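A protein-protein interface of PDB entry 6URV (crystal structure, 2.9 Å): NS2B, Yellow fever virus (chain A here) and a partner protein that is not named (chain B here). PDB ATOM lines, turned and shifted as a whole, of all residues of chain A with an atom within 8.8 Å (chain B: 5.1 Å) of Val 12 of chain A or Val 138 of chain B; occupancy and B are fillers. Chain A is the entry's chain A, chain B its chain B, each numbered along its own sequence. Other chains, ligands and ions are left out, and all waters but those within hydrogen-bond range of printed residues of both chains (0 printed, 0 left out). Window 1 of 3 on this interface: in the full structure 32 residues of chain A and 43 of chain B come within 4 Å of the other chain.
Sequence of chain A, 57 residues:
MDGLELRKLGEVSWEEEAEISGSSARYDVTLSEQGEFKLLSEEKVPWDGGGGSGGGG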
ATOM      1  N   LYS A   8      -8.062  18.169   4.016  1.00  0.00           N
ATOM      2  CA  LYS A   8      -9.106  19.175   4.035  1.00  0.00           C
ATOM      3  C   LYS A   8      -9.784  19.190   2.673  1.00  0.00           C
ATOM      4  O   LYS A   8      -9.112  19.224   1.637  1.00  0.00           O
ATOM      5  CB  LYS A   8      -8.514  20.542   4.374  1.00  0.00           C
ATOM      6  CG  LYS A   8      -9.487  21.702   4.298  1.00  0.00           C
ATOM      7  CD  LYS A   8      -9.418  22.532   5.570  1.00  0.00           C
ATOM      8  CE  LYS A   8      -9.642  24.003   5.285  1.00  0.00           C
ATOM      9  NZ  LYS A   8      -9.977  24.768   6.517  1.00  0.00           N
ATOM     10  N   LEU A   9     -11.118  19.166   2.674  1.00  0.00           N
ATOM     11  CA  LEU A   9     -11.886  19.170   1.440  1.00  0.00           C
ATOM     12  C   LEU A   9     -12.809  20.369   1.297  1.00  0.00           C
ATOM     13  O   LEU A   9     -13.286  20.633   0.189  1.00  0.00           O
ATOM     14  CB  LEU A   9     -12.723  17.888   1.329  1.00  0.00           C
ATOM     15  CG  LEU A   9     -11.853  16.631   1.318  1.00  0.00           C
ATOM     16  CD1 LEU A   9     -12.459  15.570   2.211  1.00  0.00           C
ATOM     17  CD2 LEU A   9     -11.668  16.137  -0.113  1.00  0.00           C
ATOM     18  N   GLY A  10     -13.058  21.105   2.372  1.00  0.00           N
ATOM     19  CA  GLY A  10     -13.903  22.275   2.311  1.00  0.00           C
ATOM     20  C   GLY A  10     -14.106  22.820   3.708  1.00  0.00           C
ATOM     21  O   GLY A  10     -13.497  22.347   4.671  1.00  0.00           O
ATOM     22  N   GLU A  11     -14.994  23.802   3.810  1.00  0.00           N
ATOM     23  CA  GLU A  11     -15.228  24.473   5.077  1.00  0.00           C
ATOM     24  C   GLU A  11     -16.728  24.562   5.330  1.00  0.00           C
ATOM     25  O   GLU A  11     -17.513  24.750   4.394  1.00  0.00           O
ATOM     26  CB  GLU A  11     -14.538  25.853   5.047  1.00  0.00           C
ATOM     27  CG  GLU A  11     -12.991  25.705   5.059  1.00  0.00           C
ATOM     28  CD  GLU A  11     -12.247  26.796   4.289  1.00  0.00           C
ATOM     29  OE1 GLU A  11     -11.856  26.510   3.124  1.00  0.00           O
ATOM     30  OE2 GLU A  11     -12.015  27.892   4.819  1.00  0.00           O
ATOM     31  N   VAL A  12     -17.116  24.448   6.598  1.00  0.00           N
ATOM     32  CA  VAL A  12     -18.524  24.360   6.972  1.00  0.00           C
ATOM     33  C   VAL A  12     -19.178  25.728   6.820  1.00  0.00           C
ATOM     34  O   VAL A  12     -18.700  26.732   7.359  1.00  0.00           O
ATOM     35  CB  VAL A  12     -18.668  23.820   8.404  1.00  0.00           C
ATOM     36  CG1 VAL A  12     -17.741  24.554   9.360  1.00  0.00           C
ATOM     37  CG2 VAL A  12     -20.101  23.912   8.873  1.00  0.00           C
ATOM     38  N   SER A  13     -20.270  25.769   6.064  1.00  0.00           N
ATOM     39  CA  SER A  13     -20.982  27.000   5.770  1.00  0.00           C
ATOM     40  C   SER A  13     -22.381  26.614   5.327  1.00  0.00           C
ATOM     41  O   SER A  13     -22.653  25.452   5.015  1.00  0.00           O
ATOM     42  CB  SER A  13     -20.272  27.827   4.691  1.00  0.00           C
ATOM     43  OG  SER A  13     -20.618  27.372   3.391  1.00  0.00           O
ATOM     44  N   TRP A  14     -23.263  27.600   5.292  1.00  0.00           N
ATOM     45  CA  TRP A  14     -24.593  27.428   4.732  1.00  0.00           C
ATOM     46  C   TRP A  14     -24.606  28.110   3.372  1.00  0.00           C
ATOM     47  O   TRP A  14     -24.425  29.329   3.281  1.00  0.00           O
ATOM     48  CB  TRP A  14     -25.665  28.008   5.658  1.00  0.00           C
ATOM     49  CG  TRP A  14     -27.039  28.120   5.044  1.00  0.00           C
ATOM     50  CD1 TRP A  14     -27.444  29.018   4.097  1.00  0.00           C
ATOM     51  CD2 TRP A  14     -28.192  27.322   5.352  1.00  0.00           C
ATOM     52  NE1 TRP A  14     -28.767  28.821   3.787  1.00  0.00           N
ATOM     53  CE2 TRP A  14     -29.250  27.786   4.544  1.00  0.00           C
ATOM     54  CE3 TRP A  14     -28.429  26.254   6.225  1.00  0.00           C
ATOM     55  CZ2 TRP A  14     -30.526  27.223   4.586  1.00  0.00           C
ATOM     56  CZ3 TRP A  14     -29.698  25.698   6.267  1.00  0.00           C
ATOM     57  CH2 TRP A  14     -30.730  26.185   5.452  1.00  0.00           C
ATOM     58  N   GLU A  15     -24.805  27.323   2.321  1.00  0.00           N
ATOM     59  CA  GLU A  15     -24.896  27.857   0.972  1.00  0.00           C
ATOM     60  C   GLU A  15     -26.354  28.198   0.695  1.00  0.00           C
ATOM     61  O   GLU A  15     -27.240  27.354   0.872  1.00  0.00           O
ATOM     62  CB  GLU A  15     -24.370  26.852  -0.052  1.00  0.00           C
ATOM     63  N   GLY B  18     -12.618  23.489   9.639  1.00  0.00           N
ATOM     64  CA  GLY B  18     -13.129  23.070   8.346  1.00  0.00           C
ATOM     65  C   GLY B  18     -13.439  21.585   8.349  1.00  0.00           C
ATOM     66  O   GLY B  18     -13.305  20.902   9.361  1.00  0.00           O
ATOM     67  N   ILE B  19     -13.858  21.095   7.181  1.00  0.00           N
ATOM     68  CA  ILE B  19     -14.248  19.697   7.001  1.00  0.00           C
ATOM     69  C   ILE B  19     -13.064  18.899   6.471  1.00  0.00           C
ATOM     70  O   ILE B  19     -12.483  19.246   5.435  1.00  0.00           O
ATOM     71  CB  ILE B  19     -15.455  19.575   6.057  1.00  0.00           C
ATOM     72  CG1 ILE B  19     -16.569  20.524   6.496  1.00  0.00           C
ATOM     73  CG2 ILE B  19     -15.956  18.140   6.009  1.00  0.00           C
ATOM     74  CD1 ILE B  19     -17.700  20.657   5.489  1.00  0.00           C
ATOM     75  N   GLU B  91     -35.232  24.504   8.622  1.00  0.00           N
ATOM     76  CA  GLU B  91     -34.674  23.728   7.527  1.00  0.00           C
ATOM     77  C   GLU B  91     -33.170  23.586   7.723  1.00  0.00           C
ATOM     78  O   GLU B  91     -32.486  24.530   8.126  1.00  0.00           O
ATOM     79  CB  GLU B  91     -34.978  24.394   6.186  1.00  0.00           C
ATOM     80  N   VAL B  92     -32.656  22.387   7.457  1.00  0.00           N
ATOM     81  CA  VAL B  92     -31.272  22.062   7.762  1.00  0.00           C
ATOM     82  C   VAL B  92     -30.540  21.812   6.454  1.00  0.00           C
ATOM     83  O   VAL B  92     -31.145  21.637   5.394  1.00  0.00           O
ATOM     84  CB  VAL B  92     -31.140  20.841   8.694  1.00  0.00           C
ATOM     85  CG1 VAL B  92     -32.033  21.002   9.908  1.00  0.00           C
ATOM     86  CG2 VAL B  92     -31.473  19.561   7.939  1.00  0.00           C
ATOM     87  N   GLN B  93     -29.217  21.810   6.539  1.00  0.00           N
ATOM     88  CA  GLN B  93     -28.369  21.608   5.378  1.00  0.00           C
ATOM     89  C   GLN B  93     -27.302  20.573   5.685  1.00  0.00           C
ATOM     90  O   GLN B  93     -26.696  20.593   6.759  1.00  0.00           O
ATOM     91  CB  GLN B  93     -27.710  22.923   4.959  1.00  0.00           C
ATOM     92  CG  GLN B  93     -27.486  23.068   3.472  1.00  0.00           C
ATOM     93  CD  GLN B  93     -27.716  24.484   2.998  1.00  0.00           C
ATOM     94  OE1 GLN B  93     -28.828  25.006   3.072  1.00  0.00           O
ATOM     95  NE2 GLN B  93     -26.659  25.119   2.511  1.00  0.00           N
ATOM     96  N   ILE B  95     -23.739  19.196   4.373  1.00  0.00           N
ATOM     97  CA  ILE B  95     -22.554  19.341   3.538  1.00  0.00           C
ATOM     98  C   ILE B  95     -21.983  17.938   3.375  1.00  0.00           C
ATOM     99  O   ILE B  95     -21.414  17.378   4.314  1.00  0.00           O
ATOM    100  CB  ILE B  95     -21.540  20.311   4.158  1.00  0.00           C
ATOM    101  CG1 ILE B  95     -22.253  21.539   4.723  1.00  0.00           C
ATOM    102  CG2 ILE B  95     -20.550  20.781   3.122  1.00  0.00           C
ATOM    103  CD1 ILE B  95     -22.264  21.605   6.225  1.00  0.00           C
ATOM    104  N   PRO B 136     -21.036  17.231   8.284  1.00  0.00           N
ATOM    105  CA  PRO B 136     -21.745  18.151   9.173  1.00  0.00           C
ATOM    106  C   PRO B 136     -23.133  18.491   8.660  1.00  0.00           C
ATOM    107  O   PRO B 136     -23.378  18.592   7.455  1.00  0.00           O
ATOM    108  CB  PRO B 136     -20.841  19.390   9.197  1.00  0.00           C
ATOM    109  CG  PRO B 136     -20.073  19.329   7.929  1.00  0.00           C
ATOM    110  CD  PRO B 136     -19.936  17.885   7.553  1.00  0.00           C
ATOM    111  N   ILE B 137     -24.043  18.667   9.616  1.00  0.00           N
ATOM    112  CA  ILE B 137     -25.387  19.176   9.380  1.00  0.00           C
ATOM    113  C   ILE B 137     -25.486  20.504  10.111  1.00  0.00           C
ATOM    114  O   ILE B 137     -25.197  20.577  11.310  1.00  0.00           O
ATOM    115  CB  ILE B 137     -26.462  18.188   9.871  1.00  0.00           C
ATOM    116  CG1 ILE B 137     -26.359  16.864   9.117  1.00  0.00           C
ATOM    117  CG2 ILE B 137     -27.855  18.786   9.713  1.00  0.00           C
ATOM    118  CD1 ILE B 137     -26.943  15.685   9.887  1.00  0.00           C
ATOM    119  N   VAL B 138     -25.912  21.545   9.397  1.00  0.00           N
ATOM    120  CA  VAL B 138     -25.805  22.905   9.903  1.00  0.00           C
ATOM    121  C   VAL B 138     -27.124  23.634   9.709  1.00  0.00           C
ATOM    122  O   VAL B 138     -27.916  23.303   8.828  1.00  0.00           O
ATOM    123  CB  VAL B 138     -24.667  23.670   9.200  1.00  0.00           C
ATOM    124  CG1 VAL B 138     -23.285  23.149   9.696  1.00  0.00           C
ATOM    125  CG2 VAL B 138     -24.860  23.672   7.644  1.00  0.00           C
ATOM    126  N   ASN B 139     -27.327  24.675  10.518  1.00  0.00           N
ATOM    127  CA  ASN B 139     -28.548  25.466  10.493  1.00  0.00           C
ATOM    128  C   ASN B 139     -28.347  26.706   9.621  1.00  0.00           C
ATOM    129  O   ASN B 139     -27.297  26.894   9.002  1.00  0.00           O
ATOM    130  CB  ASN B 139     -28.960  25.857  11.910  1.00  0.00           C
ATOM    131  CG  ASN B 139     -27.866  26.606  12.647  1.00  0.00           C
ATOM    132  OD1 ASN B 139     -26.878  27.024  12.050  1.00  0.00           O
ATOM    133  ND2 ASN B 139     -28.037  26.775  13.956  1.00  0.00           N
ATOM    134  N   ARG B 140     -29.364  27.573   9.570  1.00  0.00           N
ATOM    135  CA  ARG B 140     -29.293  28.723   8.673  1.00  0.00           C
ATOM    136  C   ARG B 140     -28.149  29.661   9.039  1.00  0.00           C
ATOM    137  O   ARG B 140     -27.622  30.362   8.167  1.00  0.00           O
ATOM    138  CB  ARG B 140     -30.621  29.483   8.685  1.00  0.00           C
ATOM    139  N   GLY B 142     -25.156  28.722  10.011  1.00  0.00           N
ATOM    140  CA  GLY B 142     -23.870  28.101   9.758  1.00  0.00           C
ATOM    141  C   GLY B 142     -23.204  27.396  10.925  1.00  0.00           C
ATOM    142  O   GLY B 142     -22.062  26.941  10.774  1.00  0.00           O
ATOM    143  N   GLU B 143     -23.855  27.313  12.082  1.00  0.00           N
ATOM    144  CA  GLU B 143     -23.357  26.514  13.193  1.00  0.00           C
ATOM    145  C   GLU B 143     -23.741  25.043  12.988  1.00  0.00           C
ATOM    146  O   GLU B 143     -24.783  24.724  12.401  1.00  0.00           O
ATOM    147  CB  GLU B 143     -23.903  27.048  14.512  1.00  0.00           C
ATOM    148  N   VAL B 144     -22.944  24.138  13.558  1.00  0.00           N
ATOM    149  CA  VAL B 144     -23.080  22.707  13.279  1.00  0.00           C
ATOM    150  C   VAL B 144     -24.089  22.099  14.241  1.00  0.00           C
ATOM    151  O   VAL B 144     -23.881  22.091  15.458  1.00  0.00           O
ATOM    152  CB  VAL B 144     -21.729  21.982  13.397  1.00  0.00           C
ATOM    153  CG1 VAL B 144     -21.962  20.484  13.561  1.00  0.00           C
ATOM    154  CG2 VAL B 144     -20.853  22.263  12.192  1.00  0.00           C
ATOM    155  N   ILE B 145     -25.157  21.543  13.680  1.00  0.00           N
ATOM    156  CA  ILE B 145     -26.242  20.990  14.480  1.00  0.00           C
ATOM    157  C   ILE B 145     -26.000  19.527  14.835  1.00  0.00           C
ATOM    158  O   ILE B 145     -26.451  19.063  15.887  1.00  0.00           O
ATOM    159  CB  ILE B 145     -27.566  21.157  13.712  1.00  0.00           C
ATOM    160  CG1 ILE B 145     -27.839  22.634  13.430  1.00  0.00           C
ATOM    161  CG2 ILE B 145     -28.720  20.526  14.462  1.00  0.00           C
ATOM    162  CD1 ILE B 145     -27.587  23.534  14.615  1.00  0.00           C
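NE2 of Gln 93 of chain B sits at hydrogen-bond distance from O of Glu 15 of chain A (2.8 Å).
The backbone carbonyl oxygen (O) of Ile 19 of chain B lies within hydrogen-bond range of the backbone NH (N) of Leu 9 of chain A.
The backbone NH (N) of Ile 19 of chain B is in hydrogen-bond range of the backbone carbonyl oxygen (O) of Gly 10 of chain A.
The side-chain amide oxygen (OD1) of Asn 139 of chain B sits at hydrogen-bond distance from the backbone NH (N) of Gly 142 of chain B (3.2 Å).
The backbone NH (N) of Glu 143 of chain B lies within hydrogen-bond range of the side-chain amide oxygen (OD1) of Asn 139 of chain B (3.0 Å).
O of Gln 93 of chain B lies within hydrogen-bond range of N of Val 138 of chain B, at 2.9 Å.
N of Ile 95 of chain B is in hydrogen-bond range of O of Pro 136 of chain B, 3.2 Å away.
N of Val 12 of chain A touches CG1 of Ile 19 of chain B (3.96 Å).
CG2 of Val 12 of chain A touches CG1 of Val 138 of chain B, at 3.4 Å.
Val 12 of chain A touches Val 144 of chain B (CG2 to CG2, 3.8 Å).
Ile 95 of chain B touches Ser 13 of chain A (CG1 to O, 3.9 Å).
Ser 13 of chain A touches Val 138 of chain B (O to CG2, 3.9 Å).
Glu 91 of chain B touches Trp 14 of chain A (O to CZ3, 3.5 Å).
Gln 93 of chain B touches Trp 14 of chain A.
Trp 14 of chain A touches Val 138 of chain B.
Asn 139 of chain B touches Trp 14 of chain A (O to CE3, 3.1 Å).
CE3 of Trp 14 of chain A touches CA of Arg 140 of chain B, 3.6 Å away.
Of chain B, only Ile 19 (3.96 Å), Val 138 (3.4 Å) and Val 144 (3.8 Å) come within 4 Å of Val 12 of chain A.
Val 138 of chain B touches just these residues of chain A: Val 12, Ser 13 and Trp 14.
Printed residues of chain B within 4 Å of Leu 9 of chain A: Ile 19 (3.1 Å).
Printed residues of chain A within 4 Å of Val 92 of chain B: Trp 14.
Of the printed residues of chain A, Ile 95 of chain B touches Ser 13 (3.9 Å).
Glu 11 of chain A touches none of the printed residues of chain B.
Pro 136 of chain B touches none of the printed residues of chain A.
The nearest printed residue of chain B that does not touch Gly 10 of chain A is Ile 95 of chain B (6.8 Å).
Hydrophobic or aromatic side chains of chain B that line the printed part of chain A: Ile 19, Ile 95, Val 138 and Val 144.
Hydrophobic or aromatic side chains of chain A within 4 Å of the printed part of chain B: Val 12 and Trp 14.
Among the printed residues, no Asp or Glu carboxylate lies within 4 Å of a Lys or Arg side-chain nitrogen of the other chain.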
